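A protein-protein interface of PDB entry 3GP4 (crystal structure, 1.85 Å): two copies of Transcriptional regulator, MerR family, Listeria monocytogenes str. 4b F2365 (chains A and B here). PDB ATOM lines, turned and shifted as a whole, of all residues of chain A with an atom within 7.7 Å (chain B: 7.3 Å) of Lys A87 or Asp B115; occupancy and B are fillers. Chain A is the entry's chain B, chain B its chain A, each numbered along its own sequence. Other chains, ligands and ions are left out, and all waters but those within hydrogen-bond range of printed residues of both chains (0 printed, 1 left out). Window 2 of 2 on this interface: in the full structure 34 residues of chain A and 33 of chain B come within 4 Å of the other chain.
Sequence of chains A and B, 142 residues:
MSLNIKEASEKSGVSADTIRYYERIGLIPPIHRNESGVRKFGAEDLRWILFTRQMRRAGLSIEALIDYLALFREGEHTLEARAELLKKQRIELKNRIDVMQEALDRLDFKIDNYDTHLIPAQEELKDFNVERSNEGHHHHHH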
ATOM      1  N   LEU A  79     -37.210 -15.579   1.100  1.00  0.00           N
ATOM      2  CA  LEU A  79     -36.022 -16.405   0.842  1.00  0.00           C
ATOM      3  C   LEU A  79     -34.691 -15.619   0.852  1.00  0.00           C
ATOM      4  O   LEU A  79     -33.713 -16.031   1.499  1.00  0.00           O
ATOM      5  CB  LEU A  79     -36.166 -17.162  -0.489  1.00  0.00           C
ATOM      6  CG  LEU A  79     -37.226 -18.259  -0.420  1.00  0.00           C
ATOM      7  CD1 LEU A  79     -37.566 -18.721  -1.816  1.00  0.00           C
ATOM      8  CD2 LEU A  79     -36.687 -19.422   0.391  1.00  0.00           C
ATOM      9  N   GLU A  80     -34.653 -14.501   0.128  1.00  0.00           N
ATOM     10  CA  GLU A  80     -33.450 -13.669   0.088  1.00  0.00           C
ATOM     11  C   GLU A  80     -33.093 -13.060   1.451  1.00  0.00           C
ATOM     12  O   GLU A  80     -31.901 -13.006   1.820  1.00  0.00           O
ATOM     13  CB  GLU A  80     -33.556 -12.575  -0.987  1.00  0.00           C
ATOM     14  CG  GLU A  80     -33.331 -13.185  -2.393  1.00  0.00           C
ATOM     15  CD  GLU A  80     -33.162 -12.170  -3.510  1.00  0.00           C
ATOM     16  OE1 GLU A  80     -34.171 -11.512  -3.852  1.00  0.00           O
ATOM     17  OE2 GLU A  80     -32.031 -12.060  -4.073  1.00  0.00           O
ATOM     18  N   ALA A  81     -34.087 -12.597   2.205  1.00  0.00           N
ATOM     19  CA  ALA A  81     -33.768 -12.062   3.559  1.00  0.00           C
ATOM     20  C   ALA A  81     -33.279 -13.161   4.490  1.00  0.00           C
ATOM     21  O   ALA A  81     -32.437 -12.915   5.386  1.00  0.00           O
ATOM     22  CB  ALA A  81     -34.938 -11.326   4.187  1.00  0.00           C
ATOM     23  N   ARG A  82     -33.785 -14.376   4.309  1.00  0.00           N
ATOM     24  CA  ARG A  82     -33.287 -15.508   5.133  1.00  0.00           C
ATOM     25  C   ARG A  82     -31.838 -15.905   4.836  1.00  0.00           C
ATOM     26  O   ARG A  82     -31.060 -16.192   5.768  1.00  0.00           O
ATOM     27  CB  ARG A  82     -34.216 -16.719   5.016  1.00  0.00           C
ATOM     28  CG  ARG A  82     -35.490 -16.565   5.816  1.00  0.00           C
ATOM     29  CD  ARG A  82     -36.310 -17.846   5.708  1.00  0.00           C
ATOM     30  NE  ARG A  82     -37.295 -17.776   4.610  1.00  0.00           N
ATOM     31  CZ  ARG A  82     -37.736 -18.812   3.892  1.00  0.00           C
ATOM     32  NH1 ARG A  82     -37.232 -20.051   4.036  1.00  0.00           N
ATOM     33  NH2 ARG A  82     -38.671 -18.600   2.968  1.00  0.00           N
ATOM     34  N   ALA A  83     -31.479 -15.953   3.552  1.00  0.00           N
ATOM     35  CA  ALA A  83     -30.109 -16.272   3.128  1.00  0.00           C
ATOM     36  C   ALA A  83     -29.162 -15.215   3.695  1.00  0.00           C
ATOM     37  O   ALA A  83     -28.085 -15.541   4.200  1.00  0.00           O
ATOM     38  CB  ALA A  83     -30.009 -16.327   1.588  1.00  0.00           C
ATOM     39  N   GLU A  84     -29.586 -13.963   3.642  1.00  0.00           N
ATOM     40  CA  GLU A  84     -28.804 -12.867   4.203  1.00  0.00           C
ATOM     41  C   GLU A  84     -28.640 -12.942   5.720  1.00  0.00           C
ATOM     42  O   GLU A  84     -27.527 -12.696   6.251  1.00  0.00           O
ATOM     43  CB  GLU A  84     -29.396 -11.521   3.795  1.00  0.00           C
ATOM     44  CG  GLU A  84     -29.154 -11.180   2.299  1.00  0.00           C
ATOM     45  CD  GLU A  84     -27.707 -11.396   1.808  1.00  0.00           C
ATOM     46  OE1 GLU A  84     -26.772 -10.857   2.441  1.00  0.00           O
ATOM     47  OE2 GLU A  84     -27.510 -12.095   0.775  1.00  0.00           O
ATOM     48  N   LEU A  85     -29.738 -13.243   6.416  1.00  0.00           N
ATOM     49  CA  LEU A  85     -29.659 -13.397   7.865  1.00  0.00           C
ATOM     50  C   LEU A  85     -28.658 -14.508   8.203  1.00  0.00           C
ATOM     51  O   LEU A  85     -27.803 -14.320   9.065  1.00  0.00           O
ATOM     52  CB  LEU A  85     -31.032 -13.672   8.477  1.00  0.00           C
ATOM     53  CG  LEU A  85     -31.190 -13.878   9.992  1.00  0.00           C
ATOM     54  CD1 LEU A  85     -32.685 -13.860  10.363  1.00  0.00           C
ATOM     55  CD2 LEU A  85     -30.597 -15.227  10.349  1.00  0.00           C
ATOM     56  N   LEU A  86     -28.792 -15.674   7.570  1.00  0.00           N
ATOM     57  CA  LEU A  86     -27.889 -16.794   7.864  1.00  0.00           C
ATOM     58  C   LEU A  86     -26.445 -16.481   7.503  1.00  0.00           C
ATOM     59  O   LEU A  86     -25.545 -16.926   8.213  1.00  0.00           O
ATOM     60  CB  LEU A  86     -28.300 -18.090   7.155  1.00  0.00           C
ATOM     61  CG  LEU A  86     -29.655 -18.695   7.544  1.00  0.00           C
ATOM     62  CD1 LEU A  86     -29.906 -19.943   6.747  1.00  0.00           C
ATOM     63  CD2 LEU A  86     -29.665 -18.986   9.049  1.00  0.00           C
ATOM     64  N   LYS A  87     -26.233 -15.760   6.401  1.00  0.00           N
ATOM     65  CA  LYS A  87     -24.882 -15.361   6.020  1.00  0.00           C
ATOM     66  C   LYS A  87     -24.255 -14.433   7.074  1.00  0.00           C
ATOM     67  O   LYS A  87     -23.053 -14.550   7.368  1.00  0.00           O
ATOM     68  CB  LYS A  87     -24.863 -14.716   4.659  1.00  0.00           C
ATOM     69  CG  LYS A  87     -24.856 -15.710   3.522  1.00  0.00           C
ATOM     70  CD  LYS A  87     -24.914 -14.907   2.225  1.00  0.00           C
ATOM     71  CE  LYS A  87     -25.612 -15.707   1.151  1.00  0.00           C
ATOM     72  NZ  LYS A  87     -25.767 -14.919  -0.119  1.00  0.00           N
ATOM     73  N   LYS A  88     -25.049 -13.521   7.642  1.00  0.00           N
ATOM     74  CA  LYS A  88     -24.542 -12.658   8.732  1.00  0.00           C
ATOM     75  C   LYS A  88     -24.190 -13.487   9.990  1.00  0.00           C
ATOM     76  O   LYS A  88     -23.139 -13.265  10.639  1.00  0.00           O
ATOM     77  CB  LYS A  88     -25.534 -11.544   9.061  1.00  0.00           C
ATOM     78  CG  LYS A  88     -25.701 -10.486   7.945  1.00  0.00           C
ATOM     79  CD  LYS A  88     -26.431  -9.233   8.452  1.00  0.00           C
ATOM     80  CE  LYS A  88     -26.826  -8.311   7.285  1.00  0.00           C
ATOM     81  NZ  LYS A  88     -27.560  -9.085   6.244  1.00  0.00           N
ATOM     82  N   GLN A  89     -25.057 -14.433  10.337  1.00  0.00           N
ATOM     83  CA  GLN A  89     -24.812 -15.321  11.494  1.00  0.00           C
ATOM     84  C   GLN A  89     -23.565 -16.179  11.265  1.00  0.00           C
ATOM     85  O   GLN A  89     -22.768 -16.398  12.205  1.00  0.00           O
ATOM     86  CB  GLN A  89     -26.032 -16.189  11.805  1.00  0.00           C
ATOM     87  CG  GLN A  89     -27.240 -15.336  12.296  1.00  0.00           C
ATOM     88  CD  GLN A  89     -26.894 -14.493  13.529  1.00  0.00           C
ATOM     89  OE1 GLN A  89     -26.289 -14.983  14.480  1.00  0.00           O
ATOM     90  NE2 GLN A  89     -27.255 -13.214  13.503  1.00  0.00           N
ATOM     91  N   ARG A  90     -23.391 -16.636  10.018  1.00  0.00           N
ATOM     92  CA  ARG A  90     -22.221 -17.429   9.612  1.00  0.00           C
ATOM     93  C   ARG A  90     -20.897 -16.680   9.885  1.00  0.00           C
ATOM     94  O   ARG A  90     -19.942 -17.241  10.499  1.00  0.00           O
ATOM     95  CB  ARG A  90     -22.324 -17.766   8.111  1.00  0.00           C
ATOM     96  CG  ARG A  90     -21.459 -18.974   7.648  1.00  0.00           C
ATOM     97  CD  ARG A  90     -19.957 -18.672   7.426  1.00  0.00           C
ATOM     98  NE  ARG A  90     -19.297 -19.816   6.791  1.00  0.00           N
ATOM     99  CZ  ARG A  90     -17.978 -19.966   6.623  1.00  0.00           C
ATOM    100  NH1 ARG A  90     -17.512 -21.079   6.067  1.00  0.00           N
ATOM    101  NH2 ARG A  90     -17.120 -19.027   7.021  1.00  0.00           N
ATOM    102  N   ILE A  91     -20.838 -15.436   9.408  1.00  0.00           N
ATOM    103  CA  ILE A  91     -19.639 -14.586   9.592  1.00  0.00           C
ATOM    104  C   ILE A  91     -19.363 -14.366  11.096  1.00  0.00           C
ATOM    105  O   ILE A  91     -18.198 -14.390  11.573  1.00  0.00           O
ATOM    106  CB  ILE A  91     -19.848 -13.246   8.902  1.00  0.00           C
ATOM    107  CG1 ILE A  91     -19.716 -13.445   7.374  1.00  0.00           C
ATOM    108  CG2 ILE A  91     -18.951 -12.163   9.560  1.00  0.00           C
ATOM    109  CD1 ILE A  91     -20.094 -12.261   6.558  1.00  0.00           C
ATOM    110  N   GLU A  92     -20.427 -14.080  11.832  1.00  0.00           N
ATOM    111  CA  GLU A  92     -20.272 -13.936  13.277  1.00  0.00           C
ATOM    112  C   GLU A  92     -19.771 -15.194  13.945  1.00  0.00           C
ATOM    113  O   GLU A  92     -18.907 -15.112  14.841  1.00  0.00           O
ATOM    114  CB  GLU A  92     -21.564 -13.428  13.926  1.00  0.00           C
ATOM    115  CG  GLU A  92     -21.604 -11.936  13.860  1.00  0.00           C
ATOM    116  CD  GLU A  92     -22.982 -11.374  13.814  1.00  0.00           C
ATOM    117  OE1 GLU A  92     -23.831 -11.842  14.593  1.00  0.00           O
ATOM    118  OE2 GLU A  92     -23.209 -10.463  12.990  1.00  0.00           O
ATOM    119  N   LEU A  93     -20.308 -16.349  13.545  1.00  0.00           N
ATOM    120  CA  LEU A  93     -19.913 -17.626  14.112  1.00  0.00           C
ATOM    121  C   LEU A  93     -18.456 -17.974  13.784  1.00  0.00           C
ATOM    122  O   LEU A  93     -17.715 -18.420  14.667  1.00  0.00           O
ATOM    123  CB  LEU A  93     -20.837 -18.778  13.657  1.00  0.00           C
ATOM    124  CG  LEU A  93     -20.425 -20.195  14.163  1.00  0.00           C
ATOM    125  CD1 LEU A  93     -20.175 -20.208  15.697  1.00  0.00           C
ATOM    126  CD2 LEU A  93     -21.449 -21.242  13.833  1.00  0.00           C
ATOM    127  N   LEU B 107     -24.962 -24.176   8.904  1.00  0.00           N
ATOM    128  CA  LEU B 107     -25.260 -22.892   8.263  1.00  0.00           C
ATOM    129  C   LEU B 107     -24.804 -22.831   6.840  1.00  0.00           C
ATOM    130  O   LEU B 107     -25.573 -22.374   5.990  1.00  0.00           O
ATOM    131  CB  LEU B 107     -24.678 -21.673   9.007  1.00  0.00           C
ATOM    132  CG  LEU B 107     -25.278 -21.416  10.385  1.00  0.00           C
ATOM    133  CD1 LEU B 107     -24.484 -20.291  11.083  1.00  0.00           C
ATOM    134  CD2 LEU B 107     -26.735 -21.022  10.236  1.00  0.00           C
ATOM    135  N   PHE B 109     -24.396 -25.304   4.695  1.00  0.00           N
ATOM    136  CA  PHE B 109     -25.268 -26.219   3.969  1.00  0.00           C
ATOM    137  C   PHE B 109     -26.581 -25.540   3.653  1.00  0.00           C
ATOM    138  O   PHE B 109     -27.063 -25.520   2.486  1.00  0.00           O
ATOM    139  CB  PHE B 109     -25.540 -27.461   4.807  1.00  0.00           C
ATOM    140  CG  PHE B 109     -26.414 -28.480   4.114  1.00  0.00           C
ATOM    141  CD1 PHE B 109     -25.909 -29.244   3.058  1.00  0.00           C
ATOM    142  CD2 PHE B 109     -27.740 -28.659   4.499  1.00  0.00           C
ATOM    143  CE1 PHE B 109     -26.713 -30.193   2.405  1.00  0.00           C
ATOM    144  CE2 PHE B 109     -28.565 -29.612   3.841  1.00  0.00           C
ATOM    145  CZ  PHE B 109     -28.042 -30.372   2.800  1.00  0.00           C
ATOM    146  N   LYS B 110     -27.173 -24.990   4.692  1.00  0.00           N
ATOM    147  CA  LYS B 110     -28.447 -24.274   4.531  1.00  0.00           C
ATOM    148  C   LYS B 110     -28.320 -23.064   3.598  1.00  0.00           C
ATOM    149  O   LYS B 110     -29.196 -22.836   2.726  1.00  0.00           O
ATOM    150  CB  LYS B 110     -29.002 -23.917   5.906  1.00  0.00           C
ATOM    151  CG  LYS B 110     -29.703 -25.114   6.480  1.00  0.00           C
ATOM    152  CD  LYS B 110     -29.729 -25.087   7.998  1.00  0.00           C
ATOM    153  CE  LYS B 110     -30.986 -24.457   8.463  1.00  0.00           C
ATOM    154  NZ  LYS B 110     -30.921 -23.008   8.237  1.00  0.00           N
ATOM    155  N   ILE B 111     -27.212 -22.329   3.706  1.00  0.00           N
ATOM    156  CA  ILE B 111     -26.945 -21.198   2.825  1.00  0.00           C
ATOM    157  C   ILE B 111     -26.720 -21.619   1.370  1.00  0.00           C
ATOM    158  O   ILE B 111     -27.182 -20.930   0.437  1.00  0.00           O
ATOM    159  CB  ILE B 111     -25.751 -20.344   3.321  1.00  0.00           C
ATOM    160  CG1 ILE B 111     -26.133 -19.605   4.607  1.00  0.00           C
ATOM    161  CG2 ILE B 111     -25.329 -19.321   2.245  1.00  0.00           C
ATOM    162  CD1 ILE B 111     -24.877 -19.162   5.458  1.00  0.00           C
ATOM    163  N   ASP B 112     -26.017 -22.728   1.165  1.00  0.00           N
ATOM    164  CA  ASP B 112     -25.841 -23.267  -0.207  1.00  0.00           C
ATOM    165  C   ASP B 112     -27.166 -23.686  -0.813  1.00  0.00           C
ATOM    166  O   ASP B 112     -27.387 -23.486  -2.004  1.00  0.00           O
ATOM    167  CB  ASP B 112     -24.846 -24.439  -0.259  1.00  0.00           C
ATOM    168  CG  ASP B 112     -24.860 -25.176  -1.628  1.00  0.00           C
ATOM    169  OD1 ASP B 112     -24.060 -24.786  -2.498  1.00  0.00           O
ATOM    170  OD2 ASP B 112     -25.672 -26.129  -1.827  1.00  0.00           O
ATOM    171  N   ASN B 113     -28.031 -24.311  -0.011  1.00  0.00           N
ATOM    172  CA  ASN B 113     -29.378 -24.597  -0.486  1.00  0.00           C
ATOM    173  C   ASN B 113     -30.134 -23.339  -0.956  1.00  0.00           C
ATOM    174  O   ASN B 113     -30.710 -23.350  -2.058  1.00  0.00           O
ATOM    175  CB  ASN B 113     -30.195 -25.388   0.522  1.00  0.00           C
ATOM    176  CG  ASN B 113     -31.500 -25.856  -0.060  1.00  0.00           C
ATOM    177  OD1 ASN B 113     -31.532 -26.410  -1.172  1.00  0.00           O
ATOM    178  ND2 ASN B 113     -32.596 -25.601   0.651  1.00  0.00           N
ATOM    179  N   TYR B 114     -30.094 -22.251  -0.176  1.00  0.00           N
ATOM    180  CA  TYR B 114     -30.717 -20.984  -0.600  1.00  0.00           C
ATOM    181  C   TYR B 114     -30.129 -20.431  -1.905  1.00  0.00           C
ATOM    182  O   TYR B 114     -30.872 -20.162  -2.854  1.00  0.00           O
ATOM    183  CB  TYR B 114     -30.621 -19.897   0.475  1.00  0.00           C
ATOM    184  CG  TYR B 114     -31.621 -20.002   1.607  1.00  0.00           C
ATOM    185  CD1 TYR B 114     -31.241 -20.481   2.851  1.00  0.00           C
ATOM    186  CD2 TYR B 114     -32.964 -19.604   1.437  1.00  0.00           C
ATOM    187  CE1 TYR B 114     -32.170 -20.586   3.903  1.00  0.00           C
ATOM    188  CE2 TYR B 114     -33.893 -19.712   2.481  1.00  0.00           C
ATOM    189  CZ  TYR B 114     -33.485 -20.197   3.714  1.00  0.00           C
ATOM    190  OH  TYR B 114     -34.389 -20.307   4.732  1.00  0.00           O
ATOM    191  N   ASP B 115     -28.803 -20.263  -1.946  1.00  0.00           N
ATOM    192  CA  ASP B 115     -28.127 -19.634  -3.086  1.00  0.00           C
ATOM    193  C   ASP B 115     -28.090 -20.520  -4.335  1.00  0.00           C
ATOM    194  O   ASP B 115     -28.020 -19.992  -5.447  1.00  0.00           O
ATOM    195  CB  ASP B 115     -26.672 -19.277  -2.746  1.00  0.00           C
ATOM    196  CG  ASP B 115     -26.540 -18.080  -1.813  1.00  0.00           C
ATOM    197  OD1 ASP B 115     -27.508 -17.343  -1.562  1.00  0.00           O
ATOM    198  OD2 ASP B 115     -25.424 -17.867  -1.328  1.00  0.00           O
ATOM    199  N   THR B 116     -28.094 -21.839  -4.159  1.00  0.00           N
ATOM    200  CA  THR B 116     -27.898 -22.784  -5.286  1.00  0.00           C
ATOM    201  C   THR B 116     -29.217 -23.280  -5.871  1.00  0.00           C
ATOM    202  O   THR B 116     -29.287 -23.615  -7.050  1.00  0.00           O
ATOM    203  CB  THR B 116     -27.076 -24.053  -4.892  1.00  0.00           C
ATOM    204  OG1 THR B 116     -25.711 -23.685  -4.672  1.00  0.00           O
ATOM    205  CG2 THR B 116     -27.100 -25.080  -6.022  1.00  0.00           C
ATOM    206  N   HIS B 117     -30.239 -23.352  -5.031  1.00  0.00           N
ATOM    207  CA  HIS B 117     -31.439 -24.091  -5.365  1.00  0.00           C
ATOM    208  C   HIS B 117     -32.637 -23.188  -5.265  1.00  0.00           C
ATOM    209  O   HIS B 117     -33.227 -22.857  -6.277  1.00  0.00           O
ATOM    210  CB  HIS B 117     -31.595 -25.343  -4.494  1.00  0.00           C
ATOM    211  CG  HIS B 117     -30.520 -26.370  -4.718  1.00  0.00           C
ATOM    212  ND1 HIS B 117     -30.507 -27.210  -5.810  1.00  0.00           N
ATOM    213  CD2 HIS B 117     -29.416 -26.674  -3.997  1.00  0.00           C
ATOM    214  CE1 HIS B 117     -29.437 -27.984  -5.754  1.00  0.00           C
ATOM    215  NE2 HIS B 117     -28.758 -27.677  -4.661  1.00  0.00           N
ATOM    216  N   LEU B 118     -32.942 -22.743  -4.052  1.00  0.00           N
ATOM    217  CA  LEU B 118     -34.185 -22.028  -3.767  1.00  0.00           C
ATOM    218  C   LEU B 118     -34.331 -20.636  -4.414  1.00  0.00           C
ATOM    219  O   LEU B 118     -35.378 -20.344  -5.018  1.00  0.00           O
ATOM    220  CB  LEU B 118     -34.431 -21.970  -2.244  1.00  0.00           C
ATOM    221  CG  LEU B 118     -34.419 -23.260  -1.389  1.00  0.00           C
ATOM    222  CD1 LEU B 118     -34.746 -22.969   0.080  1.00  0.00           C
ATOM    223  CD2 LEU B 118     -35.324 -24.406  -1.893  1.00  0.00           C
ATOM    224  N   ILE B 119     -33.307 -19.789  -4.319  1.00  0.00           N
ATOM    225  CA  ILE B 119     -33.350 -18.467  -4.923  1.00  0.00           C
ATOM    226  C   ILE B 119     -33.287 -18.524  -6.469  1.00  0.00           C
ATOM    227  O   ILE B 119     -34.158 -17.932  -7.136  1.00  0.00           O
ATOM    228  CB  ILE B 119     -32.304 -17.466  -4.289  1.00  0.00           C
ATOM    229  CG1 ILE B 119     -32.657 -17.175  -2.823  1.00  0.00           C
ATOM    230  CG2 ILE B 119     -32.257 -16.171  -5.053  1.00  0.00           C
ATOM    231  CD1 ILE B 119     -31.477 -16.621  -2.011  1.00  0.00           C
ATOM    232  N   PRO B 120     -32.302 -19.250  -7.051  1.00  0.00           N
ATOM    233  CA  PRO B 120     -32.350 -19.298  -8.526  1.00  0.00           C
ATOM    234  C   PRO B 120     -33.649 -19.926  -9.048  1.00  0.00           C
ATOM    235  O   PRO B 120     -34.162 -19.496 -10.096  1.00  0.00           O
ATOM    236  CB  PRO B 120     -31.126 -20.166  -8.894  1.00  0.00           C
ATOM    237  CG  PRO B 120     -30.260 -20.094  -7.686  1.00  0.00           C
ATOM    238  CD  PRO B 120     -31.210 -20.095  -6.544  1.00  0.00           C
ATOM    239  N   ALA B 121     -34.197 -20.909  -8.329  1.00  0.00           N
ATOM    240  CA  ALA B 121     -35.514 -21.441  -8.682  1.00  0.00           C
ATOM    241  C   ALA B 121     -36.587 -20.327  -8.738  1.00  0.00           C
ATOM    242  O   ALA B 121     -37.361 -20.242  -9.692  1.00  0.00           O
ATOM    243  CB  ALA B 121     -35.935 -22.557  -7.724  1.00  0.00           C
ATOM    244  N   GLU B 123     -36.025 -17.106  -9.113  1.00  0.00           N
ATOM    245  CA  GLU B 123     -35.615 -16.225 -10.219  1.00  0.00           C
ATOM    246  C   GLU B 123     -36.006 -16.753 -11.614  1.00  0.00           C
ATOM    247  O   GLU B 123     -36.526 -16.013 -12.450  1.00  0.00           O
ATOM    248  CB  GLU B 123     -34.100 -15.956 -10.123  1.00  0.00           C
ATOM    249  CG  GLU B 123     -33.808 -14.939  -9.008  1.00  0.00           C
ATOM    250  CD  GLU B 123     -32.334 -14.767  -8.707  1.00  0.00           C
ATOM    251  OE1 GLU B 123     -31.533 -15.659  -9.062  1.00  0.00           O
ATOM    252  OE2 GLU B 123     -31.975 -13.735  -8.094  1.00  0.00           O
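The side-chain carboxylate of Glu A84 is in salt-bridge range of the side-chain amino group of Lys A87 (3.4 Å). O of Tyr B114 sits at hydrogen-bond distance from N of Ile B119 (2.9 Å).
Of the 15 printed residues of chain A, 7 touch a printed residue of chain B. Of the 15 printed residues of chain B, 6 touch a printed residue of chain A. Among the printed residues, Asp or Glu carboxylates within 4 Å of a Lys or Arg side-chain nitrogen of the other chain: Lys A87 with Asp B115.
No position is printed for both chains.
Leu A85 touches none of the printed residues of chain B. Printed residues of chain B within 4 Å of Leu A86: Leu B107, Lys B110, Ile B111 and Tyr B114. Of chain B, only Ile B111 and Asp B115 come within 4 Å of Lys A87. Of the printed residues of chain A, Leu B107 touches Leu A86 (3.8 Å) and Arg A90 (3.9 Å). Printed residues of chain A within 4 Å of Lys B110: Leu A86 (3.6 Å). Asp B112 touches none of the printed residues of chain A. Asp B115 touches just one residue of chain A: Lys A87. The nearest residue of chain B that does not touch Lys A87 is Ile B119 (6.3 Å).
Among the printed residues, pairs that only touch across the chains: Leu A79 with Tyr B114 (3.5 Å), Leu A86 with Lys B110 (3.6 Å), Leu A86 with Ile B111 (3.6 Å), Leu A86 with Tyr B114 (3.7 Å), Leu A86 with Leu B107 (3.8 Å), Lys A87 with Ile B111 (3.8 Å), Ala A83 with Tyr B114 (3.8 Å), Ala A83 with Ile B119 (3.9 Å), Glu A80 with Ile B119 (3.9 Å), Arg A90 with Leu B107 (3.9 Å) and Arg A90 with Ile B111 (3.9 Å).
The side-chain amino group of Lys A87 lies within salt-bridge range of the side-chain carboxylate of Asp B115, at 3.2 Å. The guanidinium group of Arg A82 lies within hydrogen-bond range of the side-chain hydroxyl of Tyr B114.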
